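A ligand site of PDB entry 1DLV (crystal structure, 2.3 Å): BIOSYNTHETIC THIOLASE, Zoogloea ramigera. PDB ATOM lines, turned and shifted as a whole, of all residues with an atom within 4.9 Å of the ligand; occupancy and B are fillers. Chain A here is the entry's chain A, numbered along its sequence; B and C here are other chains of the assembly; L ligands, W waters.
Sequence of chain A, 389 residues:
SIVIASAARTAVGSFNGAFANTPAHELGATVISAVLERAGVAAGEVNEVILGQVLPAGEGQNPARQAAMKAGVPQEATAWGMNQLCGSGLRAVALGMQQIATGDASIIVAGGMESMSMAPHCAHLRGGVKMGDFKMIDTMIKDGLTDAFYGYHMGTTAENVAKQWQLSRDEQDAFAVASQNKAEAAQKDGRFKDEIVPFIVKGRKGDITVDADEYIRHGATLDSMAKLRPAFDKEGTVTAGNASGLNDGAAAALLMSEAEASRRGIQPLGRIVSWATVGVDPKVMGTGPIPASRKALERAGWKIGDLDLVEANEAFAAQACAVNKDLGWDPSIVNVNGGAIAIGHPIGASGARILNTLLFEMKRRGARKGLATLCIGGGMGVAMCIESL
O of Ser 244 is in hydrogen-bond range of N6 of the ligand (3.1 Å).
O15 of the ligand sits at hydrogen-bond distance from NE2 of His 153, 3.4 Å away.
NH2 of Arg 217 sits at hydrogen-bond distance from N2 of the ligand (3.3 Å).
The backbone carbonyl oxygen (O) of Leu 145 is in hydrogen-bond range of the backbone NH (N) of Met 154 (2.9 Å).
OG of Ser 244 lies within hydrogen-bond range of O of Ala 315, at 2.8 Å.
NE2 of His 345 lies within hydrogen-bond range of SG of Cys 86 (3.3 Å).
ND1 of His 153 lies within hydrogen-bond range of N of Gly 155 (2.8 Å).
The backbone NH (N) of Gly 241 is in hydrogen-bond range of the side-chain hydroxyl (OG1) of Thr 239, 3.0 Å away.
The side-chain amide oxygen (OE1) of Gln 180 is in hydrogen-bond range of the backbone NH (N) of Arg 217 (2.8 Å).
Merely in contact with the ligand: Cys 86 (3.9 Å), Leu 145 (3.5 Å), Met 154 (3.5 Å), Ser 224 (3.7 Å), Met 225 (3.8 Å), Leu 228 (3.4 Å), Phe 232 (3.7 Å), Ala 240 (3.3 Å), Gly 241 (3.6 Å), Gly 245 (3.95 Å), Leu 246 (3.8 Å), Met 285 (3.7 Å), Phe 316 (3.4 Å), His 345 (3.7 Å) and Met 131 of chain B (3.4 Å).
Hydrophobic or aromatic side chains that line the ligand: Leu 145, His 153, Met 154, Met 225, Leu 228, Phe 232, Ala 240, Leu 246, Met 285, Phe 316, His 345 and Met 131 of chain B.
Within 4 Å of the ligand: Cys 86, Leu 145, His 153, Met 154, Arg 217, Ser 224, Met 225, Leu 228, Phe 232, Ala 240, Gly 241, Ser 244, Gly 245, Leu 246, Met 285, Phe 316, His 345 and Met 131 of chain B.
Along chain A the residues within 4 Å of the ligand span positions 86 to 345.
Water W6 lies within hydrogen-bond range of a nitrogen (N1) of the ligand (2.5 Å) and the side-chain hydroxyl of Ser 224 (3.0 Å).
Water W1 lies within hydrogen-bond range of an oxygen (O15) of the ligand (2.5 Å), a ring nitrogen (NE2) of His 153 (3.0 Å) and the side-chain sulfur (SD) of Met 131 of chain B (3.7 Å).
Water W2 lies within hydrogen-bond range of O of His 345 (2.4 Å), O of Gly 245 (2.7 Å) and N7 of the ligand (3.2 Å).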
ATOM      1  N   CYS A  86      31.794 -34.520 -18.695  1.00  0.00           N
ATOM      2  CA  CYS A  86      31.329 -33.548 -19.590  1.00  0.00           C
ATOM      3  C   CYS A  86      32.181 -33.397 -20.864  1.00  0.00           C
ATOM      4  O   CYS A  86      31.411 -32.958 -21.683  1.00  0.00           O
ATOM      5  CB  CYS A  86      31.402 -32.190 -18.837  1.00  0.00           C
ATOM      6  SG  CYS A  86      29.999 -32.163 -17.654  1.00  0.00           S
ATOM      7  N   LEU A 145      27.795 -35.938 -11.105  1.00  0.00           N
ATOM      8  CA  LEU A 145      27.996 -34.579 -10.682  1.00  0.00           C
ATOM      9  C   LEU A 145      28.666 -34.320  -9.396  1.00  0.00           C
ATOM     10  O   LEU A 145      28.793 -33.145  -8.908  1.00  0.00           O
ATOM     11  CB  LEU A 145      26.625 -33.865 -10.666  1.00  0.00           C
ATOM     12  CG  LEU A 145      25.560 -34.171 -11.710  1.00  0.00           C
ATOM     13  CD1 LEU A 145      24.202 -33.721 -11.168  1.00  0.00           C
ATOM     14  CD2 LEU A 145      25.875 -33.469 -13.066  1.00  0.00           C
ATOM     15  N   HIS A 153      29.367 -31.145  -4.692  1.00  0.00           N
ATOM     16  CA  HIS A 153      28.827 -31.032  -6.053  1.00  0.00           C
ATOM     17  C   HIS A 153      29.666 -30.215  -6.969  1.00  0.00           C
ATOM     18  O   HIS A 153      30.423 -29.387  -6.570  1.00  0.00           O
ATOM     19  CB  HIS A 153      27.423 -30.449  -6.047  1.00  0.00           C
ATOM     20  CG  HIS A 153      26.569 -30.585  -7.267  1.00  0.00           C
ATOM     21  ND1 HIS A 153      26.784 -29.889  -8.452  1.00  0.00           N
ATOM     22  CD2 HIS A 153      25.460 -31.332  -7.505  1.00  0.00           C
ATOM     23  CE1 HIS A 153      25.866 -30.235  -9.350  1.00  0.00           C
ATOM     24  NE2 HIS A 153      25.060 -31.096  -8.811  1.00  0.00           N
ATOM     25  N   MET A 154      29.492 -30.439  -8.275  1.00  0.00           N
ATOM     26  CA  MET A 154      30.180 -29.719  -9.334  1.00  0.00           C
ATOM     27  C   MET A 154      29.910 -28.220  -9.134  1.00  0.00           C
ATOM     28  O   MET A 154      30.708 -27.310  -9.384  1.00  0.00           O
ATOM     29  CB  MET A 154      29.630 -30.151 -10.691  1.00  0.00           C
ATOM     30  CG  MET A 154      30.211 -31.424 -11.267  1.00  0.00           C
ATOM     31  SD  MET A 154      31.979 -31.464 -11.289  1.00  0.00           S
ATOM     32  CE  MET A 154      32.603 -32.174  -9.832  1.00  0.00           C
ATOM     33  N   GLY A 155      28.712 -27.889  -8.567  1.00  0.00           N
ATOM     34  CA  GLY A 155      28.365 -26.517  -8.249  1.00  0.00           C
ATOM     35  C   GLY A 155      29.238 -25.801  -7.185  1.00  0.00           C
ATOM     36  O   GLY A 155      29.325 -24.574  -7.205  1.00  0.00           O
ATOM     37  N   GLN A 180      20.046 -16.953 -22.004  1.00  0.00           N
ATOM     38  CA  GLN A 180      18.673 -17.293 -22.236  1.00  0.00           C
ATOM     39  C   GLN A 180      18.170 -16.486 -23.409  1.00  0.00           C
ATOM     40  O   GLN A 180      17.585 -16.912 -24.401  1.00  0.00           O
ATOM     41  CB  GLN A 180      17.749 -16.971 -20.992  1.00  0.00           C
ATOM     42  CG  GLN A 180      18.126 -17.957 -19.833  1.00  0.00           C
ATOM     43  CD  GLN A 180      17.454 -19.303 -19.986  1.00  0.00           C
ATOM     44  OE1 GLN A 180      16.782 -19.605 -20.960  1.00  0.00           O
ATOM     45  NE2 GLN A 180      17.561 -20.270 -19.057  1.00  0.00           N
ATOM     46  N   ARG A 217      14.398 -20.821 -21.708  1.00  0.00           N
ATOM     47  CA  ARG A 217      13.305 -20.057 -21.138  1.00  0.00           C
ATOM     48  C   ARG A 217      12.994 -18.798 -21.935  1.00  0.00           C
ATOM     49  O   ARG A 217      13.762 -17.922 -22.380  1.00  0.00           O
ATOM     50  CB  ARG A 217      13.203 -19.850 -19.637  1.00  0.00           C
ATOM     51  CG  ARG A 217      14.418 -19.870 -18.815  1.00  0.00           C
ATOM     52  CD  ARG A 217      14.298 -20.466 -17.455  1.00  0.00           C
ATOM     53  NE  ARG A 217      13.288 -19.862 -16.648  1.00  0.00           N
ATOM     54  CZ  ARG A 217      12.707 -20.509 -15.637  1.00  0.00           C
ATOM     55  NH1 ARG A 217      13.040 -21.750 -15.353  1.00  0.00           N
ATOM     56  NH2 ARG A 217      11.779 -19.873 -14.911  1.00  0.00           N
ATOM     57  N   SER A 224      13.696 -12.085 -11.626  1.00  0.00           N
ATOM     58  CA  SER A 224      13.394 -13.395 -11.055  1.00  0.00           C
ATOM     59  C   SER A 224      14.661 -14.230 -10.934  1.00  0.00           C
ATOM     60  O   SER A 224      14.688 -15.139 -10.081  1.00  0.00           O
ATOM     61  CB  SER A 224      12.387 -14.036 -12.003  1.00  0.00           C
ATOM     62  OG  SER A 224      13.221 -14.112 -13.184  1.00  0.00           O
ATOM     63  N   MET A 225      15.675 -13.898 -11.693  1.00  0.00           N
ATOM     64  CA  MET A 225      16.975 -14.592 -11.560  1.00  0.00           C
ATOM     65  C   MET A 225      17.614 -14.218 -10.231  1.00  0.00           C
ATOM     66  O   MET A 225      18.114 -14.957  -9.384  1.00  0.00           O
ATOM     67  CB  MET A 225      17.677 -14.092 -12.790  1.00  0.00           C
ATOM     68  CG  MET A 225      19.017 -14.204 -13.376  1.00  0.00           C
ATOM     69  SD  MET A 225      19.125 -15.785 -14.349  1.00  0.00           S
ATOM     70  CE  MET A 225      19.382 -16.649 -12.920  1.00  0.00           C
ATOM     71  N   LEU A 228      16.540 -15.791  -6.861  1.00  0.00           N
ATOM     72  CA  LEU A 228      16.748 -17.182  -6.581  1.00  0.00           C
ATOM     73  C   LEU A 228      17.701 -17.406  -5.429  1.00  0.00           C
ATOM     74  O   LEU A 228      18.488 -16.482  -5.416  1.00  0.00           O
ATOM     75  CB  LEU A 228      17.168 -18.004  -7.792  1.00  0.00           C
ATOM     76  CG  LEU A 228      16.162 -17.930  -8.922  1.00  0.00           C
ATOM     77  CD1 LEU A 228      16.874 -18.136 -10.242  1.00  0.00           C
ATOM     78  CD2 LEU A 228      14.958 -18.819  -8.579  1.00  0.00           C
ATOM     79  N   ALA A 231      22.043 -22.525  -4.529  1.00  0.00           N
ATOM     80  CA  ALA A 231      21.716 -23.940  -4.507  1.00  0.00           C
ATOM     81  C   ALA A 231      22.740 -24.841  -3.859  1.00  0.00           C
ATOM     82  O   ALA A 231      22.422 -25.962  -3.496  1.00  0.00           O
ATOM     83  CB  ALA A 231      21.579 -24.309  -6.027  1.00  0.00           C
ATOM     84  N   PHE A 232      24.028 -24.481  -3.818  1.00  0.00           N
ATOM     85  CA  PHE A 232      25.034 -25.385  -3.260  1.00  0.00           C
ATOM     86  C   PHE A 232      25.681 -24.926  -1.971  1.00  0.00           C
ATOM     87  O   PHE A 232      25.933 -25.720  -1.082  1.00  0.00           O
ATOM     88  CB  PHE A 232      26.060 -25.537  -4.388  1.00  0.00           C
ATOM     89  CG  PHE A 232      25.459 -26.145  -5.642  1.00  0.00           C
ATOM     90  CD1 PHE A 232      25.133 -27.481  -5.810  1.00  0.00           C
ATOM     91  CD2 PHE A 232      25.260 -25.265  -6.684  1.00  0.00           C
ATOM     92  CE1 PHE A 232      24.603 -27.930  -7.011  1.00  0.00           C
ATOM     93  CE2 PHE A 232      24.709 -25.702  -7.888  1.00  0.00           C
ATOM     94  CZ  PHE A 232      24.403 -27.061  -8.086  1.00  0.00           C
ATOM     95  N   THR A 239      23.208 -20.384  -8.372  1.00  0.00           N
ATOM     96  CA  THR A 239      21.819 -20.684  -8.183  1.00  0.00           C
ATOM     97  C   THR A 239      21.327 -21.594  -9.282  1.00  0.00           C
ATOM     98  O   THR A 239      22.177 -21.833 -10.135  1.00  0.00           O
ATOM     99  CB  THR A 239      20.846 -19.475  -8.132  1.00  0.00           C
ATOM    100  OG1 THR A 239      20.590 -18.989  -9.418  1.00  0.00           O
ATOM    101  CG2 THR A 239      21.254 -18.446  -7.099  1.00  0.00           C
ATOM    102  N   ALA A 240      20.034 -21.955  -9.285  1.00  0.00           N
ATOM    103  CA  ALA A 240      19.554 -22.805 -10.343  1.00  0.00           C
ATOM    104  C   ALA A 240      19.517 -22.049 -11.657  1.00  0.00           C
ATOM    105  O   ALA A 240      19.475 -22.570 -12.828  1.00  0.00           O
ATOM    106  CB  ALA A 240      18.173 -23.390 -10.250  1.00  0.00           C
ATOM    107  N   GLY A 241      19.353 -20.743 -11.490  1.00  0.00           N
ATOM    108  CA  GLY A 241      19.241 -19.933 -12.623  1.00  0.00           C
ATOM    109  C   GLY A 241      20.566 -19.688 -13.314  1.00  0.00           C
ATOM    110  O   GLY A 241      20.504 -19.399 -14.533  1.00  0.00           O
ATOM    111  N   ALA A 243      23.223 -21.788 -13.363  1.00  0.00           N
ATOM    112  CA  ALA A 243      23.891 -23.087 -13.521  1.00  0.00           C
ATOM    113  C   ALA A 243      23.213 -23.812 -14.653  1.00  0.00           C
ATOM    114  O   ALA A 243      22.071 -23.474 -14.981  1.00  0.00           O
ATOM    115  CB  ALA A 243      23.827 -23.979 -12.297  1.00  0.00           C
ATOM    116  N   SER A 244      23.923 -24.798 -15.228  1.00  0.00           N
ATOM    117  CA  SER A 244      23.379 -25.521 -16.385  1.00  0.00           C
ATOM    118  C   SER A 244      22.214 -26.349 -15.833  1.00  0.00           C
ATOM    119  O   SER A 244      22.178 -26.332 -14.643  1.00  0.00           O
ATOM    120  CB  SER A 244      24.437 -26.373 -17.040  1.00  0.00           C
ATOM    121  OG  SER A 244      25.282 -27.126 -16.231  1.00  0.00           O
ATOM    122  N   GLY A 245      21.417 -27.042 -16.604  1.00  0.00           N
ATOM    123  CA  GLY A 245      20.405 -27.900 -15.940  1.00  0.00           C
ATOM    124  C   GLY A 245      20.830 -29.353 -16.004  1.00  0.00           C
ATOM    125  O   GLY A 245      21.903 -29.784 -16.464  1.00  0.00           O
ATOM    126  N   LEU A 246      19.806 -30.141 -15.673  1.00  0.00           N
ATOM    127  CA  LEU A 246      19.886 -31.585 -15.716  1.00  0.00           C
ATOM    128  C   LEU A 246      19.173 -31.941 -16.957  1.00  0.00           C
ATOM    129  O   LEU A 246      18.050 -31.571 -17.186  1.00  0.00           O
ATOM    130  CB  LEU A 246      19.263 -32.139 -14.424  1.00  0.00           C
ATOM    131  CG  LEU A 246      19.940 -31.574 -13.178  1.00  0.00           C
ATOM    132  CD1 LEU A 246      19.073 -32.063 -11.991  1.00  0.00           C
ATOM    133  CD2 LEU A 246      21.337 -32.177 -13.013  1.00  0.00           C
ATOM    134  N   MET A 285      37.588 -27.117 -11.327  1.00  0.00           N
ATOM    135  CA  MET A 285      37.464 -27.875 -12.568  1.00  0.00           C
ATOM    136  C   MET A 285      36.986 -27.095 -13.794  1.00  0.00           C
ATOM    137  O   MET A 285      37.391 -27.332 -14.967  1.00  0.00           O
ATOM    138  CB  MET A 285      36.696 -29.160 -12.359  1.00  0.00           C
ATOM    139  CG  MET A 285      35.199 -28.869 -12.136  1.00  0.00           C
ATOM    140  SD  MET A 285      34.329 -28.847 -13.700  1.00  0.00           S
ATOM    141  CE  MET A 285      32.980 -27.795 -13.389  1.00  0.00           C
ATOM    142  N   ALA A 315      28.934 -24.702 -18.164  1.00  0.00           N
ATOM    143  CA  ALA A 315      28.664 -25.550 -16.986  1.00  0.00           C
ATOM    144  C   ALA A 315      27.940 -24.707 -15.938  1.00  0.00           C
ATOM    145  O   ALA A 315      26.942 -25.031 -15.347  1.00  0.00           O
ATOM    146  CB  ALA A 315      30.054 -26.021 -16.566  1.00  0.00           C
ATOM    147  N   PHE A 316      28.660 -23.549 -15.688  1.00  0.00           N
ATOM    148  CA  PHE A 316      28.028 -22.642 -14.689  1.00  0.00           C
ATOM    149  C   PHE A 316      28.343 -21.231 -15.178  1.00  0.00           C
ATOM    150  O   PHE A 316      29.443 -21.106 -15.751  1.00  0.00           O
ATOM    151  CB  PHE A 316      28.656 -22.759 -13.258  1.00  0.00           C
ATOM    152  CG  PHE A 316      28.333 -24.085 -12.669  1.00  0.00           C
ATOM    153  CD1 PHE A 316      27.177 -24.314 -12.022  1.00  0.00           C
ATOM    154  CD2 PHE A 316      29.226 -25.164 -12.863  1.00  0.00           C
ATOM    155  CE1 PHE A 316      26.872 -25.596 -11.546  1.00  0.00           C
ATOM    156  CE2 PHE A 316      28.949 -26.429 -12.411  1.00  0.00           C
ATOM    157  CZ  PHE A 316      27.761 -26.596 -11.723  1.00  0.00           C
ATOM    158  N   HIS A 345      22.244 -29.302 -20.477  1.00  0.00           N
ATOM    159  CA  HIS A 345      23.455 -30.020 -20.252  1.00  0.00           C
ATOM    160  C   HIS A 345      23.360 -31.527 -20.029  1.00  0.00           C
ATOM    161  O   HIS A 345      23.545 -32.034 -18.902  1.00  0.00           O
ATOM    162  CB  HIS A 345      24.161 -29.456 -19.008  1.00  0.00           C
ATOM    163  CG  HIS A 345      25.642 -29.737 -18.917  1.00  0.00           C
ATOM    164  ND1 HIS A 345      26.309 -30.382 -19.955  1.00  0.00           N
ATOM    165  CD2 HIS A 345      26.583 -29.306 -18.060  1.00  0.00           C
ATOM    166  CE1 HIS A 345      27.575 -30.389 -19.634  1.00  0.00           C
ATOM    167  NE2 HIS A 345      27.753 -29.823 -18.491  1.00  0.00           N
ATOM    168  N   ILE A 347      25.072 -34.294 -19.809  1.00  0.00           N
ATOM    169  CA  ILE A 347      26.499 -34.549 -19.694  1.00  0.00           C
ATOM    170  C   ILE A 347      27.304 -35.298 -20.753  1.00  0.00           C
ATOM    171  O   ILE A 347      28.196 -34.630 -21.258  1.00  0.00           O
ATOM    172  CB  ILE A 347      26.876 -34.985 -18.278  1.00  0.00           C
ATOM    173  CG1 ILE A 347      26.273 -36.272 -17.809  1.00  0.00           C
ATOM    174  CG2 ILE A 347      26.525 -33.756 -17.419  1.00  0.00           C
ATOM    175  CD1 ILE A 347      26.462 -36.486 -16.305  1.00  0.00           C
ATOM    176  N   CYS A 375      34.543 -27.831 -19.868  1.00  0.00           N
ATOM    177  CA  CYS A 375      35.163 -28.038 -18.552  1.00  0.00           C
ATOM    178  C   CYS A 375      34.784 -29.431 -18.078  1.00  0.00           C
ATOM    179  O   CYS A 375      33.759 -29.821 -18.609  1.00  0.00           O
ATOM    180  CB  CYS A 375      34.792 -26.965 -17.555  1.00  0.00           C
ATOM    181  SG  CYS A 375      33.154 -26.988 -16.898  1.00  0.00           S
ATOM    182  N   MET B 131      15.293 -36.441  -7.500  1.00  0.00           N
ATOM    183  CA  MET B 131      16.732 -36.218  -7.477  1.00  0.00           C
ATOM    184  C   MET B 131      17.243 -36.445  -6.045  1.00  0.00           C
ATOM    185  O   MET B 131      16.544 -36.041  -5.072  1.00  0.00           O
ATOM    186  CB  MET B 131      16.976 -34.746  -7.849  1.00  0.00           C
ATOM    187  CG  MET B 131      18.416 -34.436  -8.183  1.00  0.00           C
ATOM    188  SD  MET B 131      18.684 -32.740  -8.673  1.00  0.00           S
ATOM    189  CE  MET B 131      18.233 -31.745  -7.305  1.00  0.00           C
ATOM    190  N   LYS C 205       3.562 -24.365   0.901  1.00  0.00           N
ATOM    191  CA  LYS C 205       3.166 -23.337  -0.052  1.00  0.00           C
ATOM    192  C   LYS C 205       1.679 -23.074   0.089  1.00  0.00           C
ATOM    193  O   LYS C 205       1.005 -22.618  -0.831  1.00  0.00           O
ATOM    194  CB  LYS C 205       3.599 -23.732  -1.466  1.00  0.00           C
ATOM    195  CG  LYS C 205       4.991 -24.345  -1.577  1.00  0.00           C
ATOM    196  CD  LYS C 205       5.618 -24.256  -2.960  1.00  0.00           C
ATOM    197  CE  LYS C 205       7.084 -24.662  -2.973  1.00  0.00           C
ATOM    198  NZ  LYS C 205       7.769 -24.234  -4.240  1.00  0.00           N
HETATM  199  N1  LIG L   1      14.581 -17.549 -13.808  1.00  0.00           N
HETATM  200  C1  LIG L   1      13.579 -17.764 -12.852  1.00  0.00           C
HETATM  201  N2  LIG L   1      13.367 -18.889 -12.145  1.00  0.00           N
HETATM  202  C2  LIG L   1      14.222 -19.835 -12.497  1.00  0.00           C
HETATM  203  C3  LIG L   1      15.284 -19.765 -13.433  1.00  0.00           C
HETATM  204  C4  LIG L   1      15.471 -18.503 -14.171  1.00  0.00           C
HETATM  205  N3  LIG L   1      16.415 -18.374 -15.078  1.00  0.00           N
HETATM  206  N4  LIG L   1      15.931 -20.891 -13.538  1.00  0.00           N
HETATM  207  C5  LIG L   1      15.344 -21.750 -12.657  1.00  0.00           C
HETATM  208  N5  LIG L   1      14.323 -21.129 -11.971  1.00  0.00           N
HETATM  209  C6  LIG L   1      13.403 -21.719 -10.961  1.00  0.00           C
HETATM  210  C7  LIG L   1      12.917 -23.066 -11.416  1.00  0.00           C
HETATM  211  O1  LIG L   1      11.699 -22.855 -12.106  1.00  0.00           O
HETATM  212  C8  LIG L   1      12.460 -23.636 -10.023  1.00  0.00           C
HETATM  213  O2  LIG L   1      11.326 -22.990  -9.680  1.00  0.00           O
HETATM  214  P1  LIG L   1      10.211 -23.952  -8.829  1.00  0.00           P
HETATM  215  O3  LIG L   1       9.556 -24.911  -9.915  1.00  0.00           O
HETATM  216  O4  LIG L   1      10.985 -24.826  -7.752  1.00  0.00           O
HETATM  217  O5  LIG L   1       9.169 -22.898  -8.291  1.00  0.00           O
HETATM  218  C9  LIG L   1      13.808 -23.358  -9.307  1.00  0.00           C
HETATM  219  O6  LIG L   1      14.132 -21.943  -9.743  1.00  0.00           O
HETATM  220  C10 LIG L   1      14.950 -24.045 -10.106  1.00  0.00           C
HETATM  221  O7  LIG L   1      14.952 -25.298  -9.423  1.00  0.00           O
HETATM  222  P2  LIG L   1      14.975 -26.672 -10.242  1.00  0.00           P
HETATM  223  O8  LIG L   1      13.798 -27.410  -9.706  1.00  0.00           O
HETATM  224  O9  LIG L   1      15.155 -26.468 -11.731  1.00  0.00           O
HETATM  225  O10 LIG L   1      16.230 -27.383  -9.803  1.00  0.00           O
HETATM  226  P3  LIG L   1      16.754 -28.194  -8.484  1.00  0.00           P
HETATM  227  O11 LIG L   1      16.979 -27.337  -7.275  1.00  0.00           O
HETATM  228  O12 LIG L   1      15.966 -29.428  -8.266  1.00  0.00           O
HETATM  229  O13 LIG L   1      18.268 -28.406  -9.209  1.00  0.00           O
HETATM  230  C11 LIG L   1      20.365 -27.493  -9.557  1.00  0.00           C
HETATM  231  C12 LIG L   1      18.855 -27.106  -9.548  1.00  0.00           C
HETATM  232  C13 LIG L   1      20.578 -28.275  -8.220  1.00  0.00           C
HETATM  233  C14 LIG L   1      21.161 -26.257  -9.922  1.00  0.00           C
HETATM  234  C15 LIG L   1      20.467 -28.455 -10.815  1.00  0.00           C
HETATM  235  O14 LIG L   1      19.696 -27.976 -11.866  1.00  0.00           O
HETATM  236  C16 LIG L   1      21.883 -28.718 -11.154  1.00  0.00           C
HETATM  237  O15 LIG L   1      22.458 -29.472 -10.166  1.00  0.00           O
HETATM  238  N6  LIG L   1      22.430 -28.350 -12.271  1.00  0.00           N
HETATM  239  C17 LIG L   1      23.785 -28.773 -12.383  1.00  0.00           C
HETATM  240  C18 LIG L   1      24.507 -29.024 -13.591  1.00  0.00           C
HETATM  241  C19 LIG L   1      25.869 -29.696 -13.365  1.00  0.00           C
HETATM  242  O16 LIG L   1      26.542 -29.731 -12.279  1.00  0.00           O
HETATM  243  N7  LIG L   1      26.245 -30.258 -14.465  1.00  0.00           N
HETATM  244  C20 LIG L   1      27.585 -30.930 -14.785  1.00  0.00           C
HETATM  245  C21 LIG L   1      28.314 -29.594 -14.607  1.00  0.00           C
HETATM  246  S1  LIG L   1      30.149 -29.771 -14.600  1.00  0.00           S
HETATM  247  O   HOH W   1      22.134 -31.500  -8.711  1.00  0.00           O
HETATM  248  O   HOH W   2      24.228 -31.094 -16.758  1.00  0.00           O
HETATM  249  O   HOH W   3      14.896 -24.914 -14.090  1.00  0.00           O
HETATM  250  O   HOH W   4      20.129 -25.132 -13.201  1.00  0.00           O
HETATM  251  O   HOH W   5      11.087 -18.439 -10.059  1.00  0.00           O
HETATM  252  O   HOH W   6      14.958 -15.516 -15.182  1.00  0.00           O
